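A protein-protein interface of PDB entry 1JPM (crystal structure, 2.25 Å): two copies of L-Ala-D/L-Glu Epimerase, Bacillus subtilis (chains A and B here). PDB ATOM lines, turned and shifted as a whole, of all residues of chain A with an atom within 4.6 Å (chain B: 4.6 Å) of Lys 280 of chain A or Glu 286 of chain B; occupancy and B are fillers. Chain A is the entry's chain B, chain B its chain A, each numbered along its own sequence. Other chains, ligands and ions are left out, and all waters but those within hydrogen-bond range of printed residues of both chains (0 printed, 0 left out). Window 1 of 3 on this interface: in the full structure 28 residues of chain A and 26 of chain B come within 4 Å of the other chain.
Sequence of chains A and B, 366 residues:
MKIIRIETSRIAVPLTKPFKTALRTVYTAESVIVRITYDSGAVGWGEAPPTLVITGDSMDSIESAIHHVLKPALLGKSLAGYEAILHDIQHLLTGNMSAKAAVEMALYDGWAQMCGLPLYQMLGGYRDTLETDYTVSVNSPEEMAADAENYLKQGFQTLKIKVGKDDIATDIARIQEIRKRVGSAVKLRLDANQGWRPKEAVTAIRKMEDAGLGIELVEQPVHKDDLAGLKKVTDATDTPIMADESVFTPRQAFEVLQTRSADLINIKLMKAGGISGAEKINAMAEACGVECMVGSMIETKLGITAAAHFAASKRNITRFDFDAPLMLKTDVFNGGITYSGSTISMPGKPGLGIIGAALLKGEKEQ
The side-chain carboxylate of Glu 286 of chain B is in salt-bridge range of the side-chain amino group of Lys 280 of chain A (3.1 Å).
The side-chain amide nitrogen (ND2) of Asn 316 of chain B lies close to the backbone NH (N) of Glu 286 of chain B.
O of Met 284 of chain B sits at hydrogen-bond distance from SG of Cys 288 of chain B, 3.4 Å away.
Met 284 of chain A touches Met 284 of chain B (CE to CA, 3.9 Å).
Ala 287 of chain B touches Met 284 of chain A (CB to CE, 3.9 Å).
Lys 280 of chain A touches just one residue of chain B: Glu 286 (3.1 Å).
Printed residues of chain A within 4 Å of Glu 286 of chain B: Lys 280 (3.1 Å).
Of the printed residues of chain A, Met 284 of chain B touches Met 284 (3.9 Å).
Of the printed residues of chain B, Met 284 of chain A touches Met 284 (3.9 Å) and Ala 287 (3.9 Å).
Of the printed residues of chain A, Ala 287 of chain B touches Met 284.
Cys 288 of chain B touches none of the printed residues of chain A.
The nearest printed residue of chain A that does not touch Glu 286 of chain B is Met 284 of chain A (7.1 Å).
The nearest printed residue of chain A that does not touch Ala 287 of chain B is Pro 250 of chain A (4.7 Å).
Of the 10 printed residues of chain A, 2 touch a printed residue of chain B.
Printed residues of chain A that touch a printed residue of chain B: Lys 280 and Met 284.
Hydrophobic or aromatic side chains of chain A that line the printed part of chain B: Met 284.
Of the 10 printed residues of chain B, 3 touch a printed residue of chain A.
Printed residues of chain B that touch a printed residue of chain A: Met 284, Glu 286 and Ala 287.
Among the printed residues, 3 pairs touch across the chains.
Met 284 of chain A touches its own counterpart, Met 284 of chain B.
Of the 3 pairs that touch across the chains among the printed residues, 1 has its exchanged pair printed and touching as well.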
ATOM      1  N   PRO A 250      20.867 -16.234 -21.880  1.00  0.00           N
ATOM      2  CA  PRO A 250      19.482 -16.528 -22.260  1.00  0.00           C
ATOM      3  C   PRO A 250      19.039 -17.917 -21.804  1.00  0.00           C
ATOM      4  O   PRO A 250      17.862 -18.130 -21.496  1.00  0.00           O
ATOM      5  CB  PRO A 250      19.478 -16.353 -23.784  1.00  0.00           C
ATOM      6  CG  PRO A 250      20.912 -16.429 -24.181  1.00  0.00           C
ATOM      7  CD  PRO A 250      21.646 -15.776 -23.041  1.00  0.00           C
ATOM      8  N   SER A 276      23.625  -8.903 -28.026  1.00  0.00           N
ATOM      9  CA  SER A 276      22.951 -10.045 -28.646  1.00  0.00           C
ATOM     10  C   SER A 276      22.295 -10.889 -27.559  1.00  0.00           C
ATOM     11  O   SER A 276      21.114 -11.228 -27.646  1.00  0.00           O
ATOM     12  CB  SER A 276      23.940 -10.898 -29.460  1.00  0.00           C
ATOM     13  OG  SER A 276      25.022 -11.367 -28.668  1.00  0.00           O
ATOM     14  N   GLY A 277      23.067 -11.209 -26.527  1.00  0.00           N
ATOM     15  CA  GLY A 277      22.535 -11.999 -25.432  1.00  0.00           C
ATOM     16  C   GLY A 277      21.437 -11.246 -24.701  1.00  0.00           C
ATOM     17  O   GLY A 277      20.387 -11.815 -24.397  1.00  0.00           O
ATOM     18  N   ALA A 278      21.668  -9.963 -24.425  1.00  0.00           N
ATOM     19  CA  ALA A 278      20.675  -9.146 -23.715  1.00  0.00           C
ATOM     20  C   ALA A 278      19.344  -9.142 -24.460  1.00  0.00           C
ATOM     21  O   ALA A 278      18.281  -9.260 -23.850  1.00  0.00           O
ATOM     22  CB  ALA A 278      21.184  -7.720 -23.546  1.00  0.00           C
ATOM     23  N   GLU A 279      19.409  -9.005 -25.782  1.00  0.00           N
ATOM     24  CA  GLU A 279      18.209  -9.006 -26.614  1.00  0.00           C
ATOM     25  C   GLU A 279      17.419 -10.305 -26.495  1.00  0.00           C
ATOM     26  O   GLU A 279      16.187 -10.287 -26.418  1.00  0.00           O
ATOM     27  CB  GLU A 279      18.566  -8.823 -28.083  1.00  0.00           C
ATOM     28  CG  GLU A 279      18.652  -7.406 -28.551  1.00  0.00           C
ATOM     29  CD  GLU A 279      18.540  -7.333 -30.056  1.00  0.00           C
ATOM     30  OE1 GLU A 279      19.310  -8.048 -30.733  1.00  0.00           O
ATOM     31  OE2 GLU A 279      17.683  -6.574 -30.555  1.00  0.00           O
ATOM     32  N   LYS A 280      18.138 -11.428 -26.524  1.00  0.00           N
ATOM     33  CA  LYS A 280      17.522 -12.746 -26.426  1.00  0.00           C
ATOM     34  C   LYS A 280      16.813 -12.919 -25.088  1.00  0.00           C
ATOM     35  O   LYS A 280      15.715 -13.466 -25.029  1.00  0.00           O
ATOM     36  CB  LYS A 280      18.582 -13.849 -26.596  1.00  0.00           C
ATOM     37  CG  LYS A 280      19.144 -13.983 -28.020  1.00  0.00           C
ATOM     38  CD  LYS A 280      20.434 -14.805 -28.037  1.00  0.00           C
ATOM     39  CE  LYS A 280      21.028 -14.941 -29.445  1.00  0.00           C
ATOM     40  NZ  LYS A 280      20.446 -16.081 -30.221  1.00  0.00           N
ATOM     41  N   ILE A 281      17.448 -12.458 -24.017  1.00  0.00           N
ATOM     42  CA  ILE A 281      16.864 -12.571 -22.691  1.00  0.00           C
ATOM     43  C   ILE A 281      15.545 -11.808 -22.617  1.00  0.00           C
ATOM     44  O   ILE A 281      14.527 -12.351 -22.198  1.00  0.00           O
ATOM     45  CB  ILE A 281      17.836 -12.034 -21.622  1.00  0.00           C
ATOM     46  CG1 ILE A 281      19.071 -12.939 -21.565  1.00  0.00           C
ATOM     47  CG2 ILE A 281      17.143 -11.970 -20.245  1.00  0.00           C
ATOM     48  CD1 ILE A 281      20.145 -12.447 -20.605  1.00  0.00           C
ATOM     49  N   ASN A 282      15.555 -10.554 -23.052  1.00  0.00           N
ATOM     50  CA  ASN A 282      14.348  -9.745 -23.011  1.00  0.00           C
ATOM     51  C   ASN A 282      13.228 -10.281 -23.891  1.00  0.00           C
ATOM     52  O   ASN A 282      12.062 -10.255 -23.500  1.00  0.00           O
ATOM     53  CB  ASN A 282      14.642  -8.311 -23.427  1.00  0.00           C
ATOM     54  CG  ASN A 282      13.380  -7.483 -23.530  1.00  0.00           C
ATOM     55  OD1 ASN A 282      12.766  -7.131 -22.517  1.00  0.00           O
ATOM     56  ND2 ASN A 282      12.969  -7.186 -24.758  1.00  0.00           N
ATOM     57  N   ALA A 283      13.573 -10.748 -25.088  1.00  0.00           N
ATOM     58  CA  ALA A 283      12.570 -11.278 -26.012  1.00  0.00           C
ATOM     59  C   ALA A 283      11.911 -12.508 -25.398  1.00  0.00           C
ATOM     60  O   ALA A 283      10.701 -12.703 -25.488  1.00  0.00           O
ATOM     61  CB  ALA A 283      13.224 -11.640 -27.350  1.00  0.00           C
ATOM     62  N   MET A 284      12.737 -13.329 -24.765  1.00  0.00           N
ATOM     63  CA  MET A 284      12.304 -14.552 -24.100  1.00  0.00           C
ATOM     64  C   MET A 284      11.342 -14.186 -22.963  1.00  0.00           C
ATOM     65  O   MET A 284      10.235 -14.718 -22.862  1.00  0.00           O
ATOM     66  CB  MET A 284      13.542 -15.235 -23.544  1.00  0.00           C
ATOM     67  CG  MET A 284      13.446 -16.702 -23.285  1.00  0.00           C
ATOM     68  SD  MET A 284      15.141 -17.299 -23.050  1.00  0.00           S
ATOM     69  CE  MET A 284      15.527 -17.804 -24.692  1.00  0.00           C
ATOM     70  N   ASN B 282      13.094 -19.238 -33.129  1.00  0.00           N
ATOM     71  CA  ASN B 282      14.431 -19.739 -33.413  1.00  0.00           C
ATOM     72  C   ASN B 282      15.410 -19.449 -32.287  1.00  0.00           C
ATOM     73  O   ASN B 282      16.237 -20.299 -31.941  1.00  0.00           O
ATOM     74  CB  ASN B 282      14.958 -19.136 -34.715  1.00  0.00           C
ATOM     75  CG  ASN B 282      16.406 -19.481 -34.960  1.00  0.00           C
ATOM     76  OD1 ASN B 282      17.290 -18.633 -34.820  1.00  0.00           O
ATOM     77  ND2 ASN B 282      16.663 -20.735 -35.307  1.00  0.00           N
ATOM     78  N   ALA B 283      15.319 -18.249 -31.718  1.00  0.00           N
ATOM     79  CA  ALA B 283      16.199 -17.858 -30.620  1.00  0.00           C
ATOM     80  C   ALA B 283      15.973 -18.718 -29.365  1.00  0.00           C
ATOM     81  O   ALA B 283      16.931 -19.100 -28.695  1.00  0.00           O
ATOM     82  CB  ALA B 283      16.003 -16.370 -30.291  1.00  0.00           C
ATOM     83  N   MET B 284      14.715 -19.015 -29.039  1.00  0.00           N
ATOM     84  CA  MET B 284      14.420 -19.855 -27.874  1.00  0.00           C
ATOM     85  C   MET B 284      14.921 -21.269 -28.149  1.00  0.00           C
ATOM     86  O   MET B 284      15.528 -21.900 -27.295  1.00  0.00           O
ATOM     87  CB  MET B 284      12.921 -19.957 -27.611  1.00  0.00           C
ATOM     88  CG  MET B 284      12.184 -18.657 -27.449  1.00  0.00           C
ATOM     89  SD  MET B 284      10.451 -18.993 -27.100  1.00  0.00           S
ATOM     90  CE  MET B 284      10.093 -17.595 -26.023  1.00  0.00           C
ATOM     91  N   ALA B 285      14.629 -21.763 -29.345  1.00  0.00           N
ATOM     92  CA  ALA B 285      15.033 -23.104 -29.741  1.00  0.00           C
ATOM     93  C   ALA B 285      16.546 -23.240 -29.638  1.00  0.00           C
ATOM     94  O   ALA B 285      17.053 -24.215 -29.092  1.00  0.00           O
ATOM     95  CB  ALA B 285      14.573 -23.386 -31.170  1.00  0.00           C
ATOM     96  N   GLU B 286      17.263 -22.248 -30.158  1.00  0.00           N
ATOM     97  CA  GLU B 286      18.723 -22.264 -30.132  1.00  0.00           C
ATOM     98  C   GLU B 286      19.262 -22.287 -28.700  1.00  0.00           C
ATOM     99  O   GLU B 286      20.243 -22.977 -28.399  1.00  0.00           O
ATOM    100  CB  GLU B 286      19.271 -21.046 -30.892  1.00  0.00           C
ATOM    101  CG  GLU B 286      20.787 -20.857 -30.805  1.00  0.00           C
ATOM    102  CD  GLU B 286      21.290 -19.809 -31.785  1.00  0.00           C
ATOM    103  OE1 GLU B 286      20.719 -18.704 -31.833  1.00  0.00           O
ATOM    104  OE2 GLU B 286      22.260 -20.088 -32.512  1.00  0.00           O
ATOM    105  N   ALA B 287      18.618 -21.538 -27.812  1.00  0.00           N
ATOM    106  CA  ALA B 287      19.055 -21.504 -26.425  1.00  0.00           C
ATOM    107  C   ALA B 287      18.869 -22.882 -25.783  1.00  0.00           C
ATOM    108  O   ALA B 287      19.506 -23.193 -24.773  1.00  0.00           O
ATOM    109  CB  ALA B 287      18.264 -20.456 -25.652  1.00  0.00           C
ATOM    110  N   CYS B 288      17.998 -23.701 -26.374  1.00  0.00           N
ATOM    111  CA  CYS B 288      17.723 -25.040 -25.854  1.00  0.00           C
ATOM    112  C   CYS B 288      18.397 -26.154 -26.664  1.00  0.00           C
ATOM    113  O   CYS B 288      18.139 -27.335 -26.430  1.00  0.00           O
ATOM    114  CB  CYS B 288      16.211 -25.295 -25.815  1.00  0.00           C
ATOM    115  SG  CYS B 288      15.266 -24.181 -24.744  1.00  0.00           S
ATOM    116  N   GLY B 289      19.254 -25.786 -27.613  1.00  0.00           N
ATOM    117  CA  GLY B 289      19.926 -26.791 -28.425  1.00  0.00           C
ATOM    118  C   GLY B 289      19.002 -27.482 -29.415  1.00  0.00           C
ATOM    119  O   GLY B 289      19.243 -28.619 -29.837  1.00  0.00           O
ATOM    120  N   VAL B 290      17.935 -26.795 -29.796  1.00  0.00           N
ATOM    121  CA  VAL B 290      16.978 -27.348 -30.738  1.00  0.00           C
ATOM    122  C   VAL B 290      17.083 -26.583 -32.057  1.00  0.00           C
ATOM    123  O   VAL B 290      16.864 -25.380 -32.093  1.00  0.00           O
ATOM    124  CB  VAL B 290      15.536 -27.244 -30.163  1.00  0.00           C
ATOM    125  CG1 VAL B 290      14.507 -27.588 -31.217  1.00  0.00           C
ATOM    126  CG2 VAL B 290      15.392 -28.183 -28.974  1.00  0.00           C
ATOM    127  N   ASN B 316      21.111 -21.368 -36.377  1.00  0.00           N
ATOM    128  CA  ASN B 316      20.292 -22.450 -35.821  1.00  0.00           C
ATOM    129  C   ASN B 316      19.253 -23.039 -36.785  1.00  0.00           C
ATOM    130  O   ASN B 316      18.658 -24.070 -36.489  1.00  0.00           O
ATOM    131  CB  ASN B 316      19.594 -21.977 -34.544  1.00  0.00           C
ATOM    132  CG  ASN B 316      18.929 -23.115 -33.792  1.00  0.00           C
ATOM    133  OD1 ASN B 316      19.580 -24.100 -33.436  1.00  0.00           O
ATOM    134  ND2 ASN B 316      17.629 -22.986 -33.545  1.00  0.00           N
